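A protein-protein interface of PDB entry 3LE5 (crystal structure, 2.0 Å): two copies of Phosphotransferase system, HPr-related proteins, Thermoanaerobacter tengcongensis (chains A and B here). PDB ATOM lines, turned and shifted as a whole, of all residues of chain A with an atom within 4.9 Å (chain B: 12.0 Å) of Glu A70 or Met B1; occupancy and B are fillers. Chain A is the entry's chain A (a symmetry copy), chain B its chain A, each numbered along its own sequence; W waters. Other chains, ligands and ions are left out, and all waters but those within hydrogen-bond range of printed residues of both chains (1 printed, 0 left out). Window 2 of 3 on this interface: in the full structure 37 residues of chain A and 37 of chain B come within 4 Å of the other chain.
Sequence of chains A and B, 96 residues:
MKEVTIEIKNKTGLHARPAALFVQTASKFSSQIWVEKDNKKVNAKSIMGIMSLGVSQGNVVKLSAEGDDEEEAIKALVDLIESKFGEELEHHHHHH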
ATOM      1  N   SER A  31      15.988 -20.522  34.277  1.00  0.00           N
ATOM      2  CA  SER A  31      15.096 -19.894  33.307  1.00  0.00           C
ATOM      3  C   SER A  31      13.861 -20.744  33.092  1.00  0.00           C
ATOM      4  O   SER A  31      13.973 -21.937  32.825  1.00  0.00           O
ATOM      5  CB  SER A  31      15.802 -19.756  31.962  1.00  0.00           C
ATOM      6  OG  SER A  31      16.767 -18.728  31.996  1.00  0.00           O
ATOM      7  N   SER A  64      11.195 -20.970  23.628  1.00  0.00           N
ATOM      8  CA  SER A  64      11.435 -19.736  24.366  1.00  0.00           C
ATOM      9  C   SER A  64      11.945 -19.980  25.775  1.00  0.00           C
ATOM     10  O   SER A  64      11.656 -21.001  26.379  1.00  0.00           O
ATOM     11  CB  SER A  64      10.197 -18.826  24.376  1.00  0.00           C
ATOM     12  OG  SER A  64       9.061 -19.468  24.922  1.00  0.00           O
ATOM     13  N   ALA A  65      12.723 -19.032  26.280  1.00  0.00           N
ATOM     14  CA  ALA A  65      13.241 -19.085  27.637  1.00  0.00           C
ATOM     15  C   ALA A  65      13.243 -17.676  28.210  1.00  0.00           C
ATOM     16  O   ALA A  65      13.339 -16.701  27.474  1.00  0.00           O
ATOM     17  CB  ALA A  65      14.650 -19.672  27.653  1.00  0.00           C
ATOM     18  N   GLU A  66      13.127 -17.574  29.526  1.00  0.00           N
ATOM     19  CA  GLU A  66      13.175 -16.287  30.208  1.00  0.00           C
ATOM     20  C   GLU A  66      13.775 -16.482  31.595  1.00  0.00           C
ATOM     21  O   GLU A  66      13.156 -17.075  32.475  1.00  0.00           O
ATOM     22  CB  GLU A  66      11.775 -15.673  30.301  1.00  0.00           C
ATOM     23  CG  GLU A  66      11.748 -14.227  30.774  1.00  0.00           C
ATOM     24  CD  GLU A  66      10.477 -13.505  30.363  1.00  0.00           C
ATOM     25  OE1 GLU A  66       9.444 -14.186  30.181  1.00  0.00           O
ATOM     26  OE2 GLU A  66      10.512 -12.261  30.216  1.00  0.00           O
ATOM     27  N   GLY A  67      14.995 -16.003  31.783  1.00  0.00           N
ATOM     28  CA  GLY A  67      15.661 -16.175  33.057  1.00  0.00           C
ATOM     29  C   GLY A  67      17.102 -15.710  33.061  1.00  0.00           C
ATOM     30  O   GLY A  67      17.610 -15.194  32.060  1.00  0.00           O
ATOM     31  N   ASP A  68      17.760 -15.905  34.202  1.00  0.00           N
ATOM     32  CA  ASP A  68      19.108 -15.392  34.426  1.00  0.00           C
ATOM     33  C   ASP A  68      20.119 -16.043  33.490  1.00  0.00           C
ATOM     34  O   ASP A  68      21.249 -15.573  33.358  1.00  0.00           O
ATOM     35  CB  ASP A  68      19.526 -15.589  35.891  1.00  0.00           C
ATOM     36  CG  ASP A  68      18.654 -14.803  36.869  1.00  0.00           C
ATOM     37  OD1 ASP A  68      18.459 -13.585  36.662  1.00  0.00           O
ATOM     38  OD2 ASP A  68      18.174 -15.404  37.855  1.00  0.00           O
ATOM     39  N   ASP A  69      19.707 -17.126  32.839  1.00  0.00           N
ATOM     40  CA  ASP A  69      20.581 -17.849  31.918  1.00  0.00           C
ATOM     41  C   ASP A  69      19.839 -18.232  30.651  1.00  0.00           C
ATOM     42  O   ASP A  69      20.174 -19.230  30.014  1.00  0.00           O
ATOM     43  CB  ASP A  69      21.140 -19.112  32.581  1.00  0.00           C
ATOM     44  CG  ASP A  69      20.055 -19.970  33.227  1.00  0.00           C
ATOM     45  OD1 ASP A  69      18.858 -19.747  32.939  1.00  0.00           O
ATOM     46  OD2 ASP A  69      20.397 -20.869  34.028  1.00  0.00           O
ATOM     47  N   GLU A  70      18.837 -17.436  30.289  1.00  0.00           N
ATOM     48  CA  GLU A  70      17.969 -17.758  29.160  1.00  0.00           C
ATOM     49  C   GLU A  70      18.771 -17.942  27.876  1.00  0.00           C
ATOM     50  O   GLU A  70      18.338 -18.663  26.975  1.00  0.00           O
ATOM     51  CB  GLU A  70      16.879 -16.691  28.969  1.00  0.00           C
ATOM     52  CG  GLU A  70      17.277 -15.531  28.066  1.00  0.00           C
ATOM     53  CD  GLU A  70      16.335 -14.337  28.179  1.00  0.00           C
ATOM     54  OE1 GLU A  70      15.511 -14.317  29.114  1.00  0.00           O
ATOM     55  OE2 GLU A  70      16.420 -13.413  27.340  1.00  0.00           O
ATOM     56  N   GLU A  71      19.937 -17.303  27.799  1.00  0.00           N
ATOM     57  CA  GLU A  71      20.765 -17.370  26.596  1.00  0.00           C
ATOM     58  C   GLU A  71      21.510 -18.696  26.461  1.00  0.00           C
ATOM     59  O   GLU A  71      21.494 -19.332  25.405  1.00  0.00           O
ATOM     60  CB  GLU A  71      21.758 -16.210  26.565  1.00  0.00           C
ATOM     61  CG  GLU A  71      21.105 -14.850  26.450  1.00  0.00           C
ATOM     62  CD  GLU A  71      22.084 -13.768  26.065  1.00  0.00           C
ATOM     63  OE1 GLU A  71      23.292 -14.071  25.923  1.00  0.00           O
ATOM     64  OE2 GLU A  71      21.636 -12.613  25.897  1.00  0.00           O
ATOM     65  N   GLU A  72      22.174 -19.105  27.533  1.00  0.00           N
ATOM     66  CA  GLU A  72      22.956 -20.330  27.517  1.00  0.00           C
ATOM     67  C   GLU A  72      22.040 -21.551  27.395  1.00  0.00           C
ATOM     68  O   GLU A  72      22.407 -22.561  26.786  1.00  0.00           O
ATOM     69  CB  GLU A  72      23.832 -20.408  28.772  1.00  0.00           C
ATOM     70  CG  GLU A  72      24.947 -19.351  28.833  1.00  0.00           C
ATOM     71  CD  GLU A  72      24.448 -17.951  29.196  1.00  0.00           C
ATOM     72  OE1 GLU A  72      23.443 -17.841  29.927  1.00  0.00           O
ATOM     73  OE2 GLU A  72      25.071 -16.957  28.760  1.00  0.00           O
ATOM     74  N   ALA A  73      20.837 -21.428  27.952  1.00  0.00           N
ATOM     75  CA  ALA A  73      19.865 -22.519  27.999  1.00  0.00           C
ATOM     76  C   ALA A  73      19.230 -22.839  26.647  1.00  0.00           C
ATOM     77  O   ALA A  73      18.951 -24.003  26.345  1.00  0.00           O
ATOM     78  CB  ALA A  73      18.784 -22.216  29.031  1.00  0.00           C
ATOM     79  N   ILE A  74      18.976 -21.808  25.848  1.00  0.00           N
ATOM     80  CA  ILE A  74      18.440 -22.019  24.508  1.00  0.00           C
ATOM     81  C   ILE A  74      19.560 -22.532  23.611  1.00  0.00           C
ATOM     82  O   ILE A  74      19.347 -23.437  22.811  1.00  0.00           O
ATOM     83  CB  ILE A  74      17.765 -20.742  23.920  1.00  0.00           C
ATOM     84  CG1 ILE A  74      16.513 -20.380  24.723  1.00  0.00           C
ATOM     85  CG2 ILE A  74      17.383 -20.939  22.456  1.00  0.00           C
ATOM     86  CD1 ILE A  74      15.406 -21.402  24.620  1.00  0.00           C
ATOM     87  N   MET B   1      14.045 -12.153  27.354  1.00  0.00           N
ATOM     88  CA  MET B   1      13.524 -13.375  26.766  1.00  0.00           C
ATOM     89  C   MET B   1      14.332 -13.786  25.546  1.00  0.00           C
ATOM     90  O   MET B   1      14.859 -12.943  24.827  1.00  0.00           O
ATOM     91  CB  MET B   1      12.066 -13.196  26.366  1.00  0.00           C
ATOM     92  CG  MET B   1      11.351 -14.507  26.100  1.00  0.00           C
ATOM     93  SD  MET B   1      10.496 -14.486  24.521  1.00  0.00           S
ATOM     94  CE  MET B   1      11.874 -14.201  23.426  1.00  0.00           C
ATOM     95  N   LYS B   2      14.417 -15.091  25.317  1.00  0.00           N
ATOM     96  CA  LYS B   2      15.141 -15.624  24.181  1.00  0.00           C
ATOM     97  C   LYS B   2      14.256 -16.654  23.511  1.00  0.00           C
ATOM     98  O   LYS B   2      13.726 -17.535  24.171  1.00  0.00           O
ATOM     99  CB  LYS B   2      16.448 -16.256  24.640  1.00  0.00           C
ATOM    100  CG  LYS B   2      17.189 -17.006  23.553  1.00  0.00           C
ATOM    101  CD  LYS B   2      17.722 -16.070  22.485  1.00  0.00           C
ATOM    102  CE  LYS B   2      18.413 -16.855  21.383  1.00  0.00           C
ATOM    103  NZ  LYS B   2      19.102 -15.986  20.400  1.00  0.00           N
ATOM    104  N   GLU B   3      14.100 -16.529  22.197  1.00  0.00           N
ATOM    105  CA  GLU B   3      13.162 -17.343  21.429  1.00  0.00           C
ATOM    106  C   GLU B   3      13.779 -17.822  20.106  1.00  0.00           C
ATOM    107  O   GLU B   3      14.469 -17.062  19.433  1.00  0.00           O
ATOM    108  CB  GLU B   3      11.885 -16.527  21.168  1.00  0.00           C
ATOM    109  CG  GLU B   3      11.008 -17.016  20.014  1.00  0.00           C
ATOM    110  CD  GLU B   3       9.792 -16.120  19.751  1.00  0.00           C
ATOM    111  OE1 GLU B   3       9.134 -15.694  20.724  1.00  0.00           O
ATOM    112  OE2 GLU B   3       9.484 -15.855  18.567  1.00  0.00           O
ATOM    113  N   VAL B   4      13.541 -19.082  19.743  1.00  0.00           N
ATOM    114  CA  VAL B   4      13.953 -19.604  18.434  1.00  0.00           C
ATOM    115  C   VAL B   4      12.905 -20.553  17.855  1.00  0.00           C
ATOM    116  O   VAL B   4      12.424 -21.445  18.551  1.00  0.00           O
ATOM    117  CB  VAL B   4      15.303 -20.346  18.505  1.00  0.00           C
ATOM    118  CG1 VAL B   4      16.355 -19.462  19.119  1.00  0.00           C
ATOM    119  CG2 VAL B   4      15.178 -21.627  19.306  1.00  0.00           C
ATOM    120  N   THR B   5      12.528 -20.355  16.592  1.00  0.00           N
ATOM    121  CA  THR B   5      11.722 -21.364  15.904  1.00  0.00           C
ATOM    122  C   THR B   5      12.664 -22.259  15.126  1.00  0.00           C
ATOM    123  O   THR B   5      13.413 -21.803  14.262  1.00  0.00           O
ATOM    124  CB  THR B   5      10.637 -20.798  14.957  1.00  0.00           C
ATOM    125  OG1 THR B   5      11.239 -20.343  13.742  1.00  0.00           O
ATOM    126  CG2 THR B   5       9.849 -19.673  15.619  1.00  0.00           C
HETATM  127  O   HOH W   1      11.945 -10.362  28.758  1.00  0.00           O
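N of Met B1 sits at hydrogen-bond distance from OE2 of Glu A70, 2.7 Å away.
The backbone NH (N) of Ala A65 is in hydrogen-bond range of the backbone carbonyl oxygen (O) of Lys B2 (2.8 Å).
The backbone NH of Lys B2 lies within hydrogen-bond range of the side-chain carboxylate of Glu A70 (3.3 Å).
The side-chain hydroxyl of Ser A31 sits at hydrogen-bond distance from the backbone NH of Glu A70, at 3.0 Å.
The backbone NH (N) of Gly A67 is in hydrogen-bond range of the side-chain carboxylate (OE1) of Glu A70 (3.2 Å).
Ser A64 touches Lys B2.
Met B1 touches Ala A65 (CG to O, 3.3 Å).
Lys B2 touches Ile A74 (CG to CG1, 3.6 Å).
Ile A74 touches Val B4.
Glu A70 touches just these residues of chain B: Met B1 (2.7 Å) and Lys B2 (3.3 Å).
Of chain A, only Ala A65 (3.3 Å) and Glu A70 (2.7 Å) come within 4 Å of Met B1.
No residue of chain B comes within 4 Å of Ser A31.
Of chain B, only Lys B2 (3.2 Å) comes within 4 Å of Ser A64.
Of chain B, only Met B1 (3.3 Å) and Lys B2 (2.8 Å) come within 4 Å of Ala A65.
No residue of chain B comes within 4 Å of Glu A66.
No residue of chain B comes within 4 Å of Gly A67.
No residue of chain B comes within 4 Å of Asp A68.
No residue of chain B comes within 4 Å of Glu A71.
Ile A74 touches two residues of chain B.
Of the printed residues of chain A, Val B4 touches Ile A74.
Of the printed residues of chain A, Lys B2 touches Ser A64 (3.2 Å), Ala A65 (2.8 Å), Glu A70 (3.3 Å) and Ile A74 (3.6 Å).
Thr B5 touches none of the printed residues of chain A.
Glu B3 touches none of the printed residues of chain A.
The nearest printed residue of chain A that does not touch Lys B2 is Glu A71 (4.7 Å).
Hydrophobic or aromatic side chains of chain B that line the printed part of chain A: Met B1 and Val B4.
Of the 12 printed residues of chain A, 4 touch a printed residue of chain B.
Hydrophobic or aromatic side chains of chain A that line the printed part of chain B: Ile A74.
Among the printed residues, no Asp or Glu carboxylate lies within 4 Å of a Lys or Arg side-chain nitrogen of the other chain.
No position is printed for both chains.
Water W1 lies within hydrogen-bond range of the side-chain carboxylate (OE2) of Glu A66 (2.8 Å) and the backbone NH (N) of Met B1 (3.1 Å).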
